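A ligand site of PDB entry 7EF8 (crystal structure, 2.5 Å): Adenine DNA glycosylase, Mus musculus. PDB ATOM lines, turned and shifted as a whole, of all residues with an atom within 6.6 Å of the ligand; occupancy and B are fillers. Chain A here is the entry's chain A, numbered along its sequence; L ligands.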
ATOM      1  N   PHE A  38      28.912  -7.538 -39.045  1.00  0.00           N
ATOM      2  CA  PHE A  38      28.605  -7.373 -37.629  1.00  0.00           C
ATOM      3  C   PHE A  38      28.036  -5.991 -37.340  1.00  0.00           C
ATOM      4  O   PHE A  38      27.080  -5.855 -36.564  1.00  0.00           O
ATOM      5  CB  PHE A  38      29.857  -7.616 -36.785  1.00  0.00           C
ATOM      6  CG  PHE A  38      29.584  -7.781 -35.321  1.00  0.00           C
ATOM      7  CD1 PHE A  38      29.522  -6.678 -34.486  1.00  0.00           C
ATOM      8  CD2 PHE A  38      29.386  -9.032 -34.771  1.00  0.00           C
ATOM      9  CE1 PHE A  38      29.260  -6.819 -33.136  1.00  0.00           C
ATOM     10  CE2 PHE A  38      29.136  -9.192 -33.419  1.00  0.00           C
ATOM     11  CZ  PHE A  38      29.073  -8.085 -32.601  1.00  0.00           C
ATOM     12  N   ARG A 183      30.344  -9.486 -22.069  1.00  0.00           N
ATOM     13  CA  ARG A 183      29.637 -10.757 -22.204  1.00  0.00           C
ATOM     14  C   ARG A 183      29.392 -11.094 -23.660  1.00  0.00           C
ATOM     15  O   ARG A 183      29.528 -12.261 -24.063  1.00  0.00           O
ATOM     16  CB  ARG A 183      28.324 -10.713 -21.422  1.00  0.00           C
ATOM     17  CG  ARG A 183      27.463 -11.957 -21.577  1.00  0.00           C
ATOM     18  CD  ARG A 183      26.289 -11.967 -20.616  1.00  0.00           C
ATOM     19  NE  ARG A 183      25.476 -10.754 -20.723  1.00  0.00           N
ATOM     20  CZ  ARG A 183      25.543  -9.729 -19.870  1.00  0.00           C
ATOM     21  NH1 ARG A 183      26.397  -9.773 -18.852  1.00  0.00           N
ATOM     22  NH2 ARG A 183      24.776  -8.664 -20.048  1.00  0.00           N
ATOM     23  N   VAL A 184      29.039 -10.103 -24.478  1.00  0.00           N
ATOM     24  CA  VAL A 184      28.790 -10.355 -25.891  1.00  0.00           C
ATOM     25  C   VAL A 184      30.069 -10.798 -26.586  1.00  0.00           C
ATOM     26  O   VAL A 184      30.104 -11.800 -27.305  1.00  0.00           O
ATOM     27  CB  VAL A 184      28.177  -9.113 -26.569  1.00  0.00           C
ATOM     28  CG1 VAL A 184      28.077  -9.330 -28.070  1.00  0.00           C
ATOM     29  CG2 VAL A 184      26.818  -8.794 -25.966  1.00  0.00           C
ATOM     30  N   ARG A 187      31.518 -14.232 -25.845  1.00  0.00           N
ATOM     31  CA  ARG A 187      30.754 -15.303 -26.485  1.00  0.00           C
ATOM     32  C   ARG A 187      30.929 -15.305 -28.006  1.00  0.00           C
ATOM     33  O   ARG A 187      31.129 -16.372 -28.595  1.00  0.00           O
ATOM     34  CB  ARG A 187      29.277 -15.175 -26.129  1.00  0.00           C
ATOM     35  CG  ARG A 187      28.986 -15.390 -24.654  1.00  0.00           C
ATOM     36  CD  ARG A 187      27.519 -15.142 -24.338  1.00  0.00           C
ATOM     37  NE  ARG A 187      27.202 -15.434 -22.938  1.00  0.00           N
ATOM     38  CZ  ARG A 187      26.013 -15.234 -22.383  1.00  0.00           C
ATOM     39  NH1 ARG A 187      25.021 -14.729 -23.104  1.00  0.00           N
ATOM     40  NH2 ARG A 187      25.817 -15.537 -21.107  1.00  0.00           N
ATOM     41  N   VAL A 188      30.874 -14.132 -28.639  1.00  0.00           N
ATOM     42  CA  VAL A 188      30.983 -14.051 -30.091  1.00  0.00           C
ATOM     43  C   VAL A 188      32.311 -14.629 -30.551  1.00  0.00           C
ATOM     44  O   VAL A 188      32.371 -15.378 -31.537  1.00  0.00           O
ATOM     45  CB  VAL A 188      30.792 -12.604 -30.567  1.00  0.00           C
ATOM     46  CG1 VAL A 188      31.214 -12.454 -32.010  1.00  0.00           C
ATOM     47  CG2 VAL A 188      29.334 -12.178 -30.394  1.00  0.00           C
ATOM     48  N   LEU A 227      22.292  -4.963 -26.557  1.00  0.00           N
ATOM     49  CA  LEU A 227      22.206  -6.364 -26.958  1.00  0.00           C
ATOM     50  C   LEU A 227      22.499  -7.285 -25.782  1.00  0.00           C
ATOM     51  O   LEU A 227      21.807  -8.291 -25.586  1.00  0.00           O
ATOM     52  CB  LEU A 227      23.155  -6.641 -28.123  1.00  0.00           C
ATOM     53  CG  LEU A 227      23.030  -8.039 -28.738  1.00  0.00           C
ATOM     54  CD1 LEU A 227      21.807  -8.119 -29.644  1.00  0.00           C
ATOM     55  CD2 LEU A 227      24.304  -8.428 -29.489  1.00  0.00           C
ATOM     56  N   VAL A 231      19.256  -9.342 -25.085  1.00  0.00           N
ATOM     57  CA  VAL A 231      19.359 -10.537 -25.918  1.00  0.00           C
ATOM     58  C   VAL A 231      20.430 -11.465 -25.363  1.00  0.00           C
ATOM     59  O   VAL A 231      20.132 -12.542 -24.847  1.00  0.00           O
ATOM     60  CB  VAL A 231      19.651 -10.173 -27.387  1.00  0.00           C
ATOM     61  CG1 VAL A 231      19.898 -11.431 -28.206  1.00  0.00           C
ATOM     62  CG2 VAL A 231      18.495  -9.373 -27.970  1.00  0.00           C
ATOM     63  N   CYS A 232      21.696 -11.049 -25.454  1.00  0.00           N
ATOM     64  CA  CYS A 232      22.818 -11.811 -24.905  1.00  0.00           C
ATOM     65  C   CYS A 232      22.872 -11.641 -23.391  1.00  0.00           C
ATOM     66  O   CYS A 232      23.835 -11.121 -22.818  1.00  0.00           O
ATOM     67  CB  CYS A 232      24.119 -11.377 -25.573  1.00  0.00           C
ATOM     68  SG  CYS A 232      25.467 -12.576 -25.461  1.00  0.00           S
ATOM     69  N   THR A 233      21.810 -12.099 -22.736  1.00  0.00           N
ATOM     70  CA  THR A 233      21.660 -11.927 -21.308  1.00  0.00           C
ATOM     71  C   THR A 233      22.583 -12.879 -20.546  1.00  0.00           C
ATOM     72  O   THR A 233      23.047 -13.879 -21.100  1.00  0.00           O
ATOM     73  CB  THR A 233      20.208 -12.159 -20.901  1.00  0.00           C
ATOM     74  OG1 THR A 233      19.718 -13.351 -21.529  1.00  0.00           O
ATOM     75  CG2 THR A 233      19.340 -10.980 -21.327  1.00  0.00           C
ATOM     76  N   PRO A 237      20.117 -16.807 -22.971  1.00  0.00           N
ATOM     77  CA  PRO A 237      20.153 -15.828 -24.070  1.00  0.00           C
ATOM     78  C   PRO A 237      19.101 -16.127 -25.120  1.00  0.00           C
ATOM     79  O   PRO A 237      18.561 -17.234 -25.220  1.00  0.00           O
ATOM     80  CB  PRO A 237      21.574 -15.985 -24.633  1.00  0.00           C
ATOM     81  CG  PRO A 237      22.354 -16.678 -23.552  1.00  0.00           C
ATOM     82  CD  PRO A 237      21.363 -17.576 -22.884  1.00  0.00           C
ATOM     83  N   LEU A 238      18.815 -15.116 -25.927  1.00  0.00           N
ATOM     84  CA  LEU A 238      17.778 -15.193 -26.950  1.00  0.00           C
ATOM     85  C   LEU A 238      18.415 -15.198 -28.337  1.00  0.00           C
ATOM     86  O   LEU A 238      18.280 -14.255 -29.124  1.00  0.00           O
ATOM     87  CB  LEU A 238      16.798 -14.014 -26.793  1.00  0.00           C
ATOM     88  CG  LEU A 238      16.289 -13.738 -25.376  1.00  0.00           C
ATOM     89  CD1 LEU A 238      15.281 -12.606 -25.383  1.00  0.00           C
ATOM     90  CD2 LEU A 238      15.680 -14.987 -24.764  1.00  0.00           C
ATOM     91  N   CYS A 239      19.134 -16.285 -28.622  1.00  0.00           N
ATOM     92  CA  CYS A 239      19.776 -16.434 -29.931  1.00  0.00           C
ATOM     93  C   CYS A 239      18.759 -16.620 -31.048  1.00  0.00           C
ATOM     94  O   CYS A 239      19.090 -16.383 -32.217  1.00  0.00           O
ATOM     95  CB  CYS A 239      20.745 -17.610 -29.901  1.00  0.00           C
ATOM     96  SG  CYS A 239      21.912 -17.547 -28.534  1.00  0.00           S
ATOM     97  N   CYS A 242      18.691 -13.268 -32.018  1.00  0.00           N
ATOM     98  CA  CYS A 242      20.000 -12.627 -32.118  1.00  0.00           C
ATOM     99  C   CYS A 242      20.364 -12.336 -33.566  1.00  0.00           C
ATOM    100  O   CYS A 242      20.375 -13.235 -34.404  1.00  0.00           O
ATOM    101  CB  CYS A 242      21.074 -13.507 -31.468  1.00  0.00           C
ATOM    102  SG  CYS A 242      22.755 -12.837 -31.584  1.00  0.00           S
ATOM    103  N   PRO A 243      20.671 -11.064 -33.865  1.00  0.00           N
ATOM    104  CA  PRO A 243      21.045 -10.643 -35.219  1.00  0.00           C
ATOM    105  C   PRO A 243      22.494 -10.999 -35.550  1.00  0.00           C
ATOM    106  O   PRO A 243      22.837 -11.149 -36.726  1.00  0.00           O
ATOM    107  CB  PRO A 243      20.891  -9.122 -35.153  1.00  0.00           C
ATOM    108  CG  PRO A 243      21.169  -8.788 -33.729  1.00  0.00           C
ATOM    109  CD  PRO A 243      20.667  -9.947 -32.908  1.00  0.00           C
ATOM    110  N   VAL A 244      23.326 -11.134 -34.522  1.00  0.00           N
ATOM    111  CA  VAL A 244      24.733 -11.477 -34.715  1.00  0.00           C
ATOM    112  C   VAL A 244      25.009 -12.933 -34.373  1.00  0.00           C
ATOM    113  O   VAL A 244      26.099 -13.287 -33.954  1.00  0.00           O
ATOM    114  CB  VAL A 244      25.649 -10.578 -33.861  1.00  0.00           C
ATOM    115  CG1 VAL A 244      25.577  -9.138 -34.349  1.00  0.00           C
ATOM    116  CG2 VAL A 244      25.269 -10.675 -32.395  1.00  0.00           C
ATOM    117  N   GLN A 245      23.993 -13.772 -34.548  1.00  0.00           N
ATOM    118  CA  GLN A 245      24.119 -15.201 -34.254  1.00  0.00           C
ATOM    119  C   GLN A 245      24.939 -15.914 -35.322  1.00  0.00           C
ATOM    120  O   GLN A 245      25.380 -17.050 -35.137  1.00  0.00           O
ATOM    121  CB  GLN A 245      22.747 -15.853 -34.118  1.00  0.00           C
ATOM    122  CG  GLN A 245      22.567 -17.106 -34.949  1.00  0.00           C
ATOM    123  CD  GLN A 245      21.131 -17.595 -34.973  1.00  0.00           C
ATOM    124  OE1 GLN A 245      20.776 -18.490 -35.743  1.00  0.00           O
ATOM    125  NE2 GLN A 245      20.294 -17.011 -34.117  1.00  0.00           N
ATOM    126  N   SER A 246      25.128 -15.252 -36.463  1.00  0.00           N
ATOM    127  CA  SER A 246      25.890 -15.814 -37.564  1.00  0.00           C
ATOM    128  C   SER A 246      27.377 -15.515 -37.436  1.00  0.00           C
ATOM    129  O   SER A 246      28.197 -16.050 -38.168  1.00  0.00           O
ATOM    130  CB  SER A 246      25.358 -15.288 -38.902  1.00  0.00           C
ATOM    131  OG  SER A 246      25.626 -13.910 -39.043  1.00  0.00           O
ATOM    132  N   LEU A 247      27.711 -14.646 -36.477  1.00  0.00           N
ATOM    133  CA  LEU A 247      29.105 -14.266 -36.245  1.00  0.00           C
ATOM    134  C   LEU A 247      29.565 -14.692 -34.855  1.00  0.00           C
ATOM    135  O   LEU A 247      30.660 -14.348 -34.424  1.00  0.00           O
ATOM    136  CB  LEU A 247      29.284 -12.764 -36.429  1.00  0.00           C
ATOM    137  CG  LEU A 247      28.898 -12.184 -37.787  1.00  0.00           C
ATOM    138  CD1 LEU A 247      28.607 -10.692 -37.685  1.00  0.00           C
ATOM    139  CD2 LEU A 247      29.999 -12.447 -38.816  1.00  0.00           C
ATOM    140  N   CYS A 248      28.717 -15.451 -34.165  1.00  0.00           N
ATOM    141  CA  CYS A 248      29.042 -15.916 -32.816  1.00  0.00           C
ATOM    142  C   CYS A 248      29.622 -17.329 -32.841  1.00  0.00           C
ATOM    143  O   CYS A 248      29.006 -18.256 -33.378  1.00  0.00           O
ATOM    144  CB  CYS A 248      27.805 -15.880 -31.922  1.00  0.00           C
ATOM    145  SG  CYS A 248      28.149 -16.022 -30.157  1.00  0.00           S
ATOM    146  N   ARG A 249      30.810 -17.491 -32.275  1.00  0.00           N
ATOM    147  CA  ARG A 249      31.477 -18.782 -32.238  1.00  0.00           C
ATOM    148  C   ARG A 249      30.838 -19.702 -31.195  1.00  0.00           C
ATOM    149  O   ARG A 249      30.848 -20.923 -31.333  1.00  0.00           O
ATOM    150  CB  ARG A 249      32.967 -18.612 -31.948  1.00  0.00           C
ATOM    151  CG  ARG A 249      33.696 -17.689 -32.907  1.00  0.00           C
ATOM    152  CD  ARG A 249      33.971 -18.387 -34.226  1.00  0.00           C
ATOM    153  NE  ARG A 249      34.965 -17.668 -35.027  1.00  0.00           N
ATOM    154  CZ  ARG A 249      35.046 -17.724 -36.347  1.00  0.00           C
ATOM    155  NH1 ARG A 249      34.197 -18.471 -37.035  1.00  0.00           N
ATOM    156  NH2 ARG A 249      35.989 -17.040 -36.987  1.00  0.00           N
ATOM    157  N   ALA A 250      30.284 -19.093 -30.147  1.00  0.00           N
ATOM    158  CA  ALA A 250      29.641 -19.854 -29.080  1.00  0.00           C
ATOM    159  C   ALA A 250      28.363 -20.514 -29.575  1.00  0.00           C
ATOM    160  O   ALA A 250      28.008 -21.617 -29.155  1.00  0.00           O
ATOM    161  CB  ALA A 250      29.351 -18.954 -27.882  1.00  0.00           C
ATOM    162  N   TYR A 251      27.649 -19.831 -30.467  1.00  0.00           N
ATOM    163  CA  TYR A 251      26.403 -20.341 -31.021  1.00  0.00           C
ATOM    164  C   TYR A 251      26.661 -21.451 -32.040  1.00  0.00           C
ATOM    165  O   TYR A 251      25.957 -22.467 -32.049  1.00  0.00           O
ATOM    166  CB  TYR A 251      25.603 -19.213 -31.668  1.00  0.00           C
ATOM    167  CG  TYR A 251      24.278 -19.663 -32.228  1.00  0.00           C
ATOM    168  CD1 TYR A 251      23.146 -19.747 -31.414  1.00  0.00           C
ATOM    169  CD2 TYR A 251      24.142 -20.034 -33.564  1.00  0.00           C
ATOM    170  CE1 TYR A 251      21.932 -20.180 -31.923  1.00  0.00           C
ATOM    171  CE2 TYR A 251      22.935 -20.462 -34.079  1.00  0.00           C
ATOM    172  CZ  TYR A 251      21.827 -20.529 -33.257  1.00  0.00           C
ATOM    173  OH  TYR A 251      20.629 -20.949 -33.753  1.00  0.00           O
ATOM    174  N   VAL A 294      25.929 -21.628 -24.741  1.00  0.00           N
ATOM    175  CA  VAL A 294      26.809 -20.489 -24.988  1.00  0.00           C
ATOM    176  C   VAL A 294      27.168 -19.765 -23.707  1.00  0.00           C
ATOM    177  O   VAL A 294      28.128 -18.981 -23.684  1.00  0.00           O
ATOM    178  CB  VAL A 294      26.160 -19.515 -25.991  1.00  0.00           C
ATOM    179  CG1 VAL A 294      25.823 -20.227 -27.289  1.00  0.00           C
ATOM    180  CG2 VAL A 294      24.914 -18.899 -25.394  1.00  0.00           C
ATOM    181  N   ALA A 295      26.434 -20.006 -22.616  1.00  0.00           N
ATOM    182  CA  ALA A 295      26.727 -19.382 -21.336  1.00  0.00           C
ATOM    183  C   ALA A 295      27.980 -19.946 -20.680  1.00  0.00           C
ATOM    184  O   ALA A 295      28.309 -19.513 -19.570  1.00  0.00           O
ATOM    185  CB  ALA A 295      25.533 -19.517 -20.387  1.00  0.00           C
HETATM  186 FE1  LIG L   1      23.779 -13.763 -29.759  1.00  0.00          FE
HETATM  187 FE2  LIG L   1      24.963 -13.907 -27.308  1.00  0.00          FE
HETATM  188 FE3  LIG L   1      26.068 -15.208 -29.434  1.00  0.00          FE
HETATM  189 FE4  LIG L   1      23.733 -16.110 -28.352  1.00  0.00          FE
HETATM  190  S1  LIG L   1      25.772 -16.033 -27.338  1.00  0.00           S
HETATM  191  S2  LIG L   1      24.202 -15.855 -30.564  1.00  0.00           S
HETATM  192  S3  LIG L   1      22.738 -14.147 -27.761  1.00  0.00           S
HETATM  193  S4  LIG L   1      25.823 -12.958 -29.185  1.00  0.00           S
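The side-chain sulfur (SG) of Cys 242 binds an iron atom (FE1) of the ligand (2.3 Å).
The side-chain sulfur (SG) of Cys 239 binds an iron atom (FE4) of the ligand (2.3 Å).
SG of Cys 232 is bound to FE2 of the ligand.
The side-chain sulfur of Cys 248 binds an iron atom (FE3) of the ligand (2.3 Å).
The side-chain sulfur of Cys 242 lies close to the backbone NH of Val 244, 3.4 Å away.
The guanidinium group (NH1) of Arg 187 sits close to the side-chain sulfur (SG) of Cys 232.
O of Leu 227 sits at hydrogen-bond distance from N of Cys 232 (2.8 Å).
The backbone carbonyl oxygen of Cys 232 is in hydrogen-bond range of the guanidinium group of Arg 183.
SG of Cys 248 lies close to O of Arg 187, 3.4 Å away.
NH1 of Arg 187 sits at hydrogen-bond distance from O of Thr 233 (2.9 Å).
N of Leu 238 lies within hydrogen-bond range of O of Val 231 (3.1 Å).
OG1 of Thr 233 lies within hydrogen-bond range of O of Val 231, at 3.4 Å.
Merely in contact with the ligand: Arg 187, Val 188, Val 231, Pro 237, Val 244, Gln 245, Tyr 251 and Val 294.
Hydrophobic or aromatic side chains within 4 Å of the ligand: Val 188, Val 231, Pro 237, Val 244, Tyr 251 and Val 294.
Within 4 Å of the ligand: Arg 187, Val 188, Val 231, Cys 232, Pro 237, Cys 239, Cys 242, Val 244, Gln 245, Cys 248, Tyr 251 and Val 294.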
